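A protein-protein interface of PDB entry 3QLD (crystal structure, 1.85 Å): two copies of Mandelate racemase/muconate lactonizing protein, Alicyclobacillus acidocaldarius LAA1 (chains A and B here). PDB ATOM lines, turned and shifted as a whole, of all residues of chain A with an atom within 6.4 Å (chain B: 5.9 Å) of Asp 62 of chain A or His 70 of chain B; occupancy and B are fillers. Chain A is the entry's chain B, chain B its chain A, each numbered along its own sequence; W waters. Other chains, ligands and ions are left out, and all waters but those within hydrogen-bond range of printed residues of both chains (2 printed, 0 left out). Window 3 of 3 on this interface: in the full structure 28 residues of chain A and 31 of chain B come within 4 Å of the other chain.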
ATOM      1  N   ARG A  10       4.830   5.459  -9.832  1.00  0.00           N
ATOM      2  CA  ARG A  10       5.572   5.295  -8.616  1.00  0.00           C
ATOM      3  C   ARG A  10       4.978   4.108  -7.855  1.00  0.00           C
ATOM      4  O   ARG A  10       3.803   4.085  -7.627  1.00  0.00           O
ATOM      5  CB  ARG A  10       5.366   6.572  -7.793  1.00  0.00           C
ATOM      6  CG  ARG A  10       6.446   6.600  -6.695  1.00  0.00           C
ATOM      7  CD  ARG A  10       6.639   7.966  -6.047  1.00  0.00           C
ATOM      8  NE  ARG A  10       7.330   7.711  -4.777  1.00  0.00           N
ATOM      9  CZ  ARG A  10       8.035   8.639  -4.143  1.00  0.00           C
ATOM     10  NH1 ARG A  10       8.108   9.863  -4.652  1.00  0.00           N
ATOM     11  NH2 ARG A  10       8.652   8.332  -2.995  1.00  0.00           N
ATOM     12  N   GLN A  30      10.785   1.642  -2.946  1.00  0.00           N
ATOM     13  CA  GLN A  30      10.093   2.662  -3.775  1.00  0.00           C
ATOM     14  C   GLN A  30      10.815   2.697  -5.085  1.00  0.00           C
ATOM     15  O   GLN A  30      12.046   2.774  -5.098  1.00  0.00           O
ATOM     16  CB  GLN A  30      10.171   4.036  -3.134  1.00  0.00           C
ATOM     17  CG  GLN A  30       9.386   4.182  -1.835  1.00  0.00           C
ATOM     18  CD  GLN A  30       9.566   5.564  -1.285  1.00  0.00           C
ATOM     19  OE1 GLN A  30       9.888   6.485  -2.034  1.00  0.00           O
ATOM     20  NE2 GLN A  30       9.412   5.717  -0.003  1.00  0.00           N
ATOM     21  N   ILE A  32      10.359   3.911  -9.470  1.00  0.00           N
ATOM     22  CA  ILE A  32       9.646   4.635 -10.449  1.00  0.00           C
ATOM     23  C   ILE A  32       9.782   3.808 -11.754  1.00  0.00           C
ATOM     24  O   ILE A  32      10.952   3.564 -12.190  1.00  0.00           O
ATOM     25  CB  ILE A  32      10.255   5.999 -10.700  1.00  0.00           C
ATOM     26  CG1 ILE A  32      10.047   6.882  -9.439  1.00  0.00           C
ATOM     27  CG2 ILE A  32       9.508   6.676 -11.896  1.00  0.00           C
ATOM     28  CD1 ILE A  32      10.758   8.273  -9.530  1.00  0.00           C
ATOM     29  N   LEU A  51      17.346   5.245  -5.067  1.00  0.00           N
ATOM     30  CA  LEU A  51      16.810   4.625  -3.846  1.00  0.00           C
ATOM     31  C   LEU A  51      15.932   5.646  -3.054  1.00  0.00           C
ATOM     32  O   LEU A  51      15.872   6.799  -3.363  1.00  0.00           O
ATOM     33  CB  LEU A  51      17.967   4.110  -3.005  1.00  0.00           C
ATOM     34  CG  LEU A  51      18.842   3.006  -3.660  1.00  0.00           C
ATOM     35  CD1 LEU A  51      19.985   2.654  -2.730  1.00  0.00           C
ATOM     36  CD2 LEU A  51      18.029   1.740  -3.992  1.00  0.00           C
ATOM     37  N   ALA A  52      15.229   5.203  -2.007  1.00  0.00           N
ATOM     38  CA  ALA A  52      14.290   6.132  -1.351  1.00  0.00           C
ATOM     39  C   ALA A  52      15.001   7.335  -0.684  1.00  0.00           C
ATOM     40  O   ALA A  52      14.399   8.451  -0.587  1.00  0.00           O
ATOM     41  CB  ALA A  52      13.491   5.314  -0.257  1.00  0.00           C
ATOM     42  N   GLU A  53      16.215   7.104  -0.151  1.00  0.00           N
ATOM     43  CA  GLU A  53      16.995   8.137   0.556  1.00  0.00           C
ATOM     44  C   GLU A  53      18.303   8.313  -0.186  1.00  0.00           C
ATOM     45  O   GLU A  53      18.822   7.317  -0.726  1.00  0.00           O
ATOM     46  CB  GLU A  53      17.343   7.687   1.990  1.00  0.00           C
ATOM     47  CG  GLU A  53      16.140   7.653   2.941  1.00  0.00           C
ATOM     48  CD  GLU A  53      15.513   9.051   3.159  1.00  0.00           C
ATOM     49  OE1 GLU A  53      16.187  10.070   3.025  1.00  0.00           O
ATOM     50  OE2 GLU A  53      14.296   9.133   3.363  1.00  0.00           O
ATOM     51  N   CYS A  60      17.271  10.376  -5.266  1.00  0.00           N
ATOM     52  CA  CYS A  60      16.382   9.527  -4.447  1.00  0.00           C
ATOM     53  C   CYS A  60      15.027   9.590  -5.179  1.00  0.00           C
ATOM     54  O   CYS A  60      14.885  10.380  -6.174  1.00  0.00           O
ATOM     55  CB  CYS A  60      16.297  10.073  -2.965  1.00  0.00           C
ATOM     56  SG  CYS A  60      15.514  11.659  -2.828  1.00  0.00           S
ATOM     57  N   THR A  61      14.054   8.752  -4.775  1.00  0.00           N
ATOM     58  CA  THR A  61      12.819   8.593  -5.555  1.00  0.00           C
ATOM     59  C   THR A  61      12.127   9.949  -5.612  1.00  0.00           C
ATOM     60  O   THR A  61      11.643  10.351  -6.647  1.00  0.00           O
ATOM     61  CB  THR A  61      11.914   7.535  -4.878  1.00  0.00           C
ATOM     62  OG1 THR A  61      12.755   6.453  -4.461  1.00  0.00           O
ATOM     63  CG2 THR A  61      10.871   6.999  -5.813  1.00  0.00           C
ATOM     64  N   ASP A  62      12.134  10.703  -4.522  1.00  0.00           N
ATOM     65  CA  ASP A  62      11.349  11.912  -4.549  1.00  0.00           C
ATOM     66  C   ASP A  62      11.917  12.887  -5.565  1.00  0.00           C
ATOM     67  O   ASP A  62      11.160  13.620  -6.225  1.00  0.00           O
ATOM     68  CB  ASP A  62      11.411  12.664  -3.184  1.00  0.00           C
ATOM     69  CG  ASP A  62      10.442  12.108  -2.147  1.00  0.00           C
ATOM     70  OD1 ASP A  62       9.484  11.372  -2.512  1.00  0.00           O
ATOM     71  OD2 ASP A  62      10.732  12.402  -0.961  1.00  0.00           O
ATOM     72  N   THR A  63      13.247  13.005  -5.591  1.00  0.00           N
ATOM     73  CA  THR A  63      13.829  14.059  -6.447  1.00  0.00           C
ATOM     74  C   THR A  63      13.838  13.564  -7.909  1.00  0.00           C
ATOM     75  O   THR A  63      13.673  14.341  -8.834  1.00  0.00           O
ATOM     76  CB  THR A  63      15.267  14.490  -6.046  1.00  0.00           C
ATOM     77  OG1 THR A  63      16.135  13.348  -6.079  1.00  0.00           O
ATOM     78  CG2 THR A  63      15.279  15.126  -4.681  1.00  0.00           C
ATOM     79  N   ALA A  64      14.072  12.277  -8.108  1.00  0.00           N
ATOM     80  CA  ALA A  64      13.891  11.679  -9.421  1.00  0.00           C
ATOM     81  C   ALA A  64      12.522  11.924 -10.057  1.00  0.00           C
ATOM     82  O   ALA A  64      12.430  12.243 -11.276  1.00  0.00           O
ATOM     83  CB  ALA A  64      14.194  10.096  -9.360  1.00  0.00           C
ATOM     84  N   TRP A  65      11.462  11.710  -9.270  1.00  0.00           N
ATOM     85  CA  TRP A  65      10.094  12.002  -9.725  1.00  0.00           C
ATOM     86  C   TRP A  65       9.968  13.420 -10.285  1.00  0.00           C
ATOM     87  O   TRP A  65       9.516  13.596 -11.392  1.00  0.00           O
ATOM     88  CB  TRP A  65       9.096  11.810  -8.559  1.00  0.00           C
ATOM     89  CG  TRP A  65       7.649  11.947  -9.007  1.00  0.00           C
ATOM     90  CD1 TRP A  65       6.865  13.026  -8.867  1.00  0.00           C
ATOM     91  CD2 TRP A  65       6.830  10.922  -9.634  1.00  0.00           C
ATOM     92  NE1 TRP A  65       5.601  12.765  -9.374  1.00  0.00           N
ATOM     93  CE2 TRP A  65       5.551  11.493  -9.861  1.00  0.00           C
ATOM     94  CE3 TRP A  65       7.086   9.627 -10.085  1.00  0.00           C
ATOM     95  CZ2 TRP A  65       4.472  10.774 -10.454  1.00  0.00           C
ATOM     96  CZ3 TRP A  65       5.977   8.861 -10.668  1.00  0.00           C
ATOM     97  CH2 TRP A  65       4.722   9.461 -10.851  1.00  0.00           C
ATOM     98  N   VAL A  66      10.311  14.474  -9.509  1.00  0.00           N
ATOM     99  CA  VAL A  66      10.131  15.804 -10.092  1.00  0.00           C
ATOM    100  C   VAL A  66      11.112  16.132 -11.180  1.00  0.00           C
ATOM    101  O   VAL A  66      10.799  16.907 -12.054  1.00  0.00           O
ATOM    102  CB  VAL A  66      10.125  16.915  -8.943  1.00  0.00           C
ATOM    103  CG1 VAL A  66       9.046  16.581  -7.897  1.00  0.00           C
ATOM    104  CG2 VAL A  66      11.479  16.880  -8.238  1.00  0.00           C
ATOM    105  N   MET A  67      12.297  15.556 -11.144  1.00  0.00           N
ATOM    106  CA  MET A  67      13.258  15.726 -12.217  1.00  0.00           C
ATOM    107  C   MET A  67      12.632  15.146 -13.541  1.00  0.00           C
ATOM    108  O   MET A  67      12.689  15.757 -14.599  1.00  0.00           O
ATOM    109  CB  MET A  67      14.581  15.072 -11.797  1.00  0.00           C
ATOM    110  CG  MET A  67      15.531  14.816 -12.969  1.00  0.00           C
ATOM    111  SD  MET A  67      16.293  16.578 -13.646  1.00  0.00           S
ATOM    112  CE  MET A  67      16.489  17.564 -11.957  1.00  0.00           C
ATOM    113  N   TRP B  65      13.626  21.624  -3.309  1.00  0.00           N
ATOM    114  CA  TRP B  65      12.428  21.797  -2.470  1.00  0.00           C
ATOM    115  C   TRP B  65      12.073  20.468  -1.828  1.00  0.00           C
ATOM    116  O   TRP B  65      11.916  20.342  -0.596  1.00  0.00           O
ATOM    117  CB  TRP B  65      11.292  22.324  -3.363  1.00  0.00           C
ATOM    118  CG  TRP B  65       9.990  22.476  -2.567  1.00  0.00           C
ATOM    119  CD1 TRP B  65       8.927  21.564  -2.467  1.00  0.00           C
ATOM    120  CD2 TRP B  65       9.665  23.568  -1.718  1.00  0.00           C
ATOM    121  NE1 TRP B  65       7.961  22.075  -1.591  1.00  0.00           N
ATOM    122  CE2 TRP B  65       8.386  23.301  -1.140  1.00  0.00           C
ATOM    123  CE3 TRP B  65      10.329  24.783  -1.403  1.00  0.00           C
ATOM    124  CZ2 TRP B  65       7.749  24.212  -0.274  1.00  0.00           C
ATOM    125  CZ3 TRP B  65       9.686  25.681  -0.555  1.00  0.00           C
ATOM    126  CH2 TRP B  65       8.419  25.392  -0.011  1.00  0.00           C
ATOM    127  N   VAL B  66      11.994  19.395  -2.625  1.00  0.00           N
ATOM    128  CA  VAL B  66      11.620  18.103  -2.022  1.00  0.00           C
ATOM    129  C   VAL B  66      12.684  17.496  -1.162  1.00  0.00           C
ATOM    130  O   VAL B  66      12.397  16.763  -0.249  1.00  0.00           O
ATOM    131  CB  VAL B  66      11.082  17.025  -3.098  1.00  0.00           C
ATOM    132  CG1 VAL B  66       9.835  17.553  -3.762  1.00  0.00           C
ATOM    133  CG2 VAL B  66      12.121  16.677  -4.132  1.00  0.00           C
ATOM    134  N   MET B  67      13.946  17.723  -1.517  1.00  0.00           N
ATOM    135  CA  MET B  67      15.064  17.310  -0.691  1.00  0.00           C
ATOM    136  C   MET B  67      14.884  17.995   0.694  1.00  0.00           C
ATOM    137  O   MET B  67      15.020  17.337   1.737  1.00  0.00           O
ATOM    138  CB  MET B  67      16.372  17.699  -1.443  1.00  0.00           C
ATOM    139  CG  MET B  67      17.731  17.363  -0.768  1.00  0.00           C
ATOM    140  SD  MET B  67      18.011  15.543  -0.149  1.00  0.00           S
ATOM    141  CE  MET B  67      17.377  14.726  -1.720  1.00  0.00           C
ATOM    142  N   LEU B  68      14.585  19.282   0.689  1.00  0.00           N
ATOM    143  CA  LEU B  68      14.463  20.010   2.014  1.00  0.00           C
ATOM    144  C   LEU B  68      13.274  19.506   2.842  1.00  0.00           C
ATOM    145  O   LEU B  68      13.422  19.070   3.964  1.00  0.00           O
ATOM    146  CB  LEU B  68      14.375  21.520   1.782  1.00  0.00           C
ATOM    147  CG  LEU B  68      15.723  22.100   1.368  1.00  0.00           C
ATOM    148  CD1 LEU B  68      15.529  23.459   0.699  1.00  0.00           C
ATOM    149  CD2 LEU B  68      16.748  22.181   2.575  1.00  0.00           C
ATOM    150  N   VAL B  69      12.105  19.503   2.228  1.00  0.00           N
ATOM    151  CA  VAL B  69      10.880  19.065   2.895  1.00  0.00           C
ATOM    152  C   VAL B  69      10.919  17.642   3.378  1.00  0.00           C
ATOM    153  O   VAL B  69      10.540  17.392   4.542  1.00  0.00           O
ATOM    154  CB  VAL B  69       9.675  19.289   1.940  1.00  0.00           C
ATOM    155  CG1 VAL B  69       8.314  18.679   2.489  1.00  0.00           C
ATOM    156  CG2 VAL B  69       9.530  20.776   1.540  1.00  0.00           C
ATOM    157  N   HIS B  70      11.318  16.696   2.505  1.00  0.00           N
ATOM    158  CA  HIS B  70      11.093  15.301   2.817  1.00  0.00           C
ATOM    159  C   HIS B  70      12.330  14.595   3.368  1.00  0.00           C
ATOM    160  O   HIS B  70      12.201  13.462   3.842  1.00  0.00           O
ATOM    161  CB  HIS B  70      10.462  14.570   1.599  1.00  0.00           C
ATOM    162  CG  HIS B  70       9.102  15.088   1.237  1.00  0.00           C
ATOM    163  ND1 HIS B  70       7.984  14.836   2.018  1.00  0.00           N
ATOM    164  CD2 HIS B  70       8.671  15.865   0.210  1.00  0.00           C
ATOM    165  CE1 HIS B  70       6.929  15.407   1.473  1.00  0.00           C
ATOM    166  NE2 HIS B  70       7.318  16.068   0.393  1.00  0.00           N
ATOM    167  N   HIS B  71      13.509  15.238   3.336  1.00  0.00           N
ATOM    168  CA  HIS B  71      14.726  14.586   3.755  1.00  0.00           C
ATOM    169  C   HIS B  71      15.634  15.323   4.727  1.00  0.00           C
ATOM    170  O   HIS B  71      15.996  14.772   5.807  1.00  0.00           O
ATOM    171  CB  HIS B  71      15.557  14.178   2.525  1.00  0.00           C
ATOM    172  CG  HIS B  71      14.793  13.305   1.598  1.00  0.00           C
ATOM    173  ND1 HIS B  71      14.763  11.931   1.749  1.00  0.00           N
ATOM    174  CD2 HIS B  71      13.865  13.608   0.646  1.00  0.00           C
ATOM    175  CE1 HIS B  71      13.930  11.413   0.846  1.00  0.00           C
ATOM    176  NE2 HIS B  71      13.351  12.407   0.185  1.00  0.00           N
ATOM    177  N   LEU B  72      16.000  16.548   4.356  1.00  0.00           N
ATOM    178  CA  LEU B  72      16.948  17.313   5.156  1.00  0.00           C
ATOM    179  C   LEU B  72      16.306  17.933   6.404  1.00  0.00           C
ATOM    180  O   LEU B  72      16.838  17.747   7.485  1.00  0.00           O
ATOM    181  CB  LEU B  72      17.667  18.386   4.307  1.00  0.00           C
ATOM    182  CG  LEU B  72      18.370  17.888   3.057  1.00  0.00           C
ATOM    183  CD1 LEU B  72      19.282  19.051   2.570  1.00  0.00           C
ATOM    184  CD2 LEU B  72      19.199  16.670   3.392  1.00  0.00           C
ATOM    185  N   VAL B  73      15.146  18.579   6.260  1.00  0.00           N
ATOM    186  CA  VAL B  73      14.489  19.182   7.457  1.00  0.00           C
ATOM    187  C   VAL B  73      14.140  18.127   8.497  1.00  0.00           C
ATOM    188  O   VAL B  73      14.434  18.337   9.712  1.00  0.00           O
ATOM    189  CB  VAL B  73      13.361  20.184   7.073  1.00  0.00           C
ATOM    190  CG1 VAL B  73      12.612  20.719   8.340  1.00  0.00           C
ATOM    191  CG2 VAL B  73      13.994  21.315   6.324  1.00  0.00           C
ATOM    192  N   PRO B  74      13.622  16.946   8.080  1.00  0.00           N
ATOM    193  CA  PRO B  74      13.398  15.908   9.096  1.00  0.00           C
ATOM    194  C   PRO B  74      14.662  15.471   9.798  1.00  0.00           C
ATOM    195  O   PRO B  74      14.667  15.252  11.028  1.00  0.00           O
ATOM    196  CB  PRO B  74      12.782  14.769   8.288  1.00  0.00           C
ATOM    197  CG  PRO B  74      11.968  15.528   7.269  1.00  0.00           C
ATOM    198  CD  PRO B  74      13.006  16.548   6.794  1.00  0.00           C
ATOM    199  N   ARG B  75      15.752  15.398   9.065  1.00  0.00           N
ATOM    200  CA  ARG B  75      17.018  14.968   9.641  1.00  0.00           C
ATOM    201  C   ARG B  75      17.521  15.992  10.613  1.00  0.00           C
ATOM    202  O   ARG B  75      18.157  15.615  11.630  1.00  0.00           O
ATOM    203  CB  ARG B  75      18.081  14.720   8.573  1.00  0.00           C
ATOM    204  CG  ARG B  75      17.989  13.297   7.940  1.00  0.00           C
ATOM    205  CD  ARG B  75      19.013  13.310   6.802  1.00  0.00           C
ATOM    206  NE  ARG B  75      19.134  11.996   6.213  1.00  0.00           N
ATOM    207  CZ  ARG B  75      18.270  11.451   5.357  1.00  0.00           C
ATOM    208  NH1 ARG B  75      17.165  12.108   5.003  1.00  0.00           N
ATOM    209  NH2 ARG B  75      18.515  10.206   4.885  1.00  0.00           N
ATOM    210  N   TRP B 373       5.946  26.182   3.235  1.00  0.00           N
ATOM    211  CA  TRP B 373       5.821  24.991   4.058  1.00  0.00           C
ATOM    212  C   TRP B 373       6.435  25.244   5.438  1.00  0.00           C
ATOM    213  O   TRP B 373       7.566  25.662   5.520  1.00  0.00           O
ATOM    214  CB  TRP B 373       6.532  23.833   3.374  1.00  0.00           C
ATOM    215  CG  TRP B 373       6.543  22.539   4.129  1.00  0.00           C
ATOM    216  CD1 TRP B 373       5.546  21.606   4.168  1.00  0.00           C
ATOM    217  CD2 TRP B 373       7.628  22.016   4.902  1.00  0.00           C
ATOM    218  NE1 TRP B 373       5.949  20.537   4.946  1.00  0.00           N
ATOM    219  CE2 TRP B 373       7.235  20.757   5.377  1.00  0.00           C
ATOM    220  CE3 TRP B 373       8.916  22.500   5.235  1.00  0.00           C
ATOM    221  CZ2 TRP B 373       8.059  19.974   6.180  1.00  0.00           C
ATOM    222  CZ3 TRP B 373       9.734  21.725   6.013  1.00  0.00           C
ATOM    223  CH2 TRP B 373       9.299  20.460   6.485  1.00  0.00           C
HETATM  224  O   HOH W   1      12.496   9.741  -1.821  1.00  0.00           O
HETATM  225  O   HOH W   2      14.022  11.246   4.767  1.00  0.00           O
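A ring nitrogen (ND1) of His 71 of chain B sits at hydrogen-bond distance from the side-chain carboxylate of Glu 53 of chain A (2.7 Å). NE2 of His 71 of chain B sits at hydrogen-bond distance from SG of Cys 60 of chain A. NE2 of His 71 of chain B sits at hydrogen-bond distance from OD2 of Asp 62 of chain A. NH2 of Arg 75 of chain B lies within salt-bridge range of OE1 of Glu 53 of chain A (3.0 Å).
The backbone carbonyl oxygen of Met 67 of chain B lies within hydrogen-bond range of the backbone NH of Leu 72 of chain B (2.9 Å). The backbone carbonyl oxygen (O) of His 71 of chain B lies within hydrogen-bond range of the guanidinium group (NH1) of Arg 75 of chain B. The guanidinium group (NH1) of Arg 10 of chain A is in salt-bridge range of the side-chain carboxylate (OD1) of Asp 62 of chain A (3.0 Å). The backbone carbonyl oxygen of Cys 60 of chain A is in hydrogen-bond range of the side-chain hydroxyl of Thr 63 of chain A.
Ala 52 of chain A touches His 71 of chain B (O to CE1, 3.3 Å). CE of Met 67 of chain B touches SG of Cys 60 of chain A, at 3.8 Å. O of Asp 62 of chain A touches CG2 of Val 66 of chain B, 3.8 Å away. His 70 of chain B touches Asp 62 of chain A (CB to OD2, 3.4 Å). Val 66 of chain B touches Thr 63 of chain A (CG2 to CG2, 3.6 Å). Thr 63 of chain A touches Met 67 of chain B.
Printed residues of chain B within 4 Å of Glu 53 of chain A: His 71 and Arg 75. Of chain B, only Val 66, His 70 and His 71 come within 4 Å of Asp 62 of chain A. Of the printed residues of chain A, Val 66 of chain B touches Asp 62 and Thr 63. His 70 of chain B touches just one residue of chain A: Asp 62. The nearest printed residue of chain B that does not touch Asp 62 of chain A is Met 67 of chain B (5.9 Å). The nearest residue of chain A that does not touch His 70 of chain B is Glu 53 of chain A (4.8 Å).
Hydrophobic or aromatic side chains of chain B within 4 Å of the printed part of chain A: Val 66, Met 67, His 70 and His 71. Among the printed residues, 10 pairs touch across the chains. Among the printed residues, Asp or Glu carboxylates within 4 Å of a Lys or Arg side-chain nitrogen of the other chain: Glu 53 of chain A with Arg 75 of chain B (3.0 Å).
3 positions are printed for both chains.
Water W2 lies within hydrogen-bond range of OE2 of Glu 53 of chain A, O of His 70 of chain B, ND1 of His 71 of chain B and NH1 of Arg 75 of chain B. Water W1 lies within hydrogen-bond range of O of Ala 52 of chain A (2.6 Å), N of Asp 62 of chain A (2.9 Å), NE2 of His 71 of chain B (3.4 Å), N of Thr 61 of chain A (3.5 Å) and SG of Cys 60 of chain A (3.7 Å).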
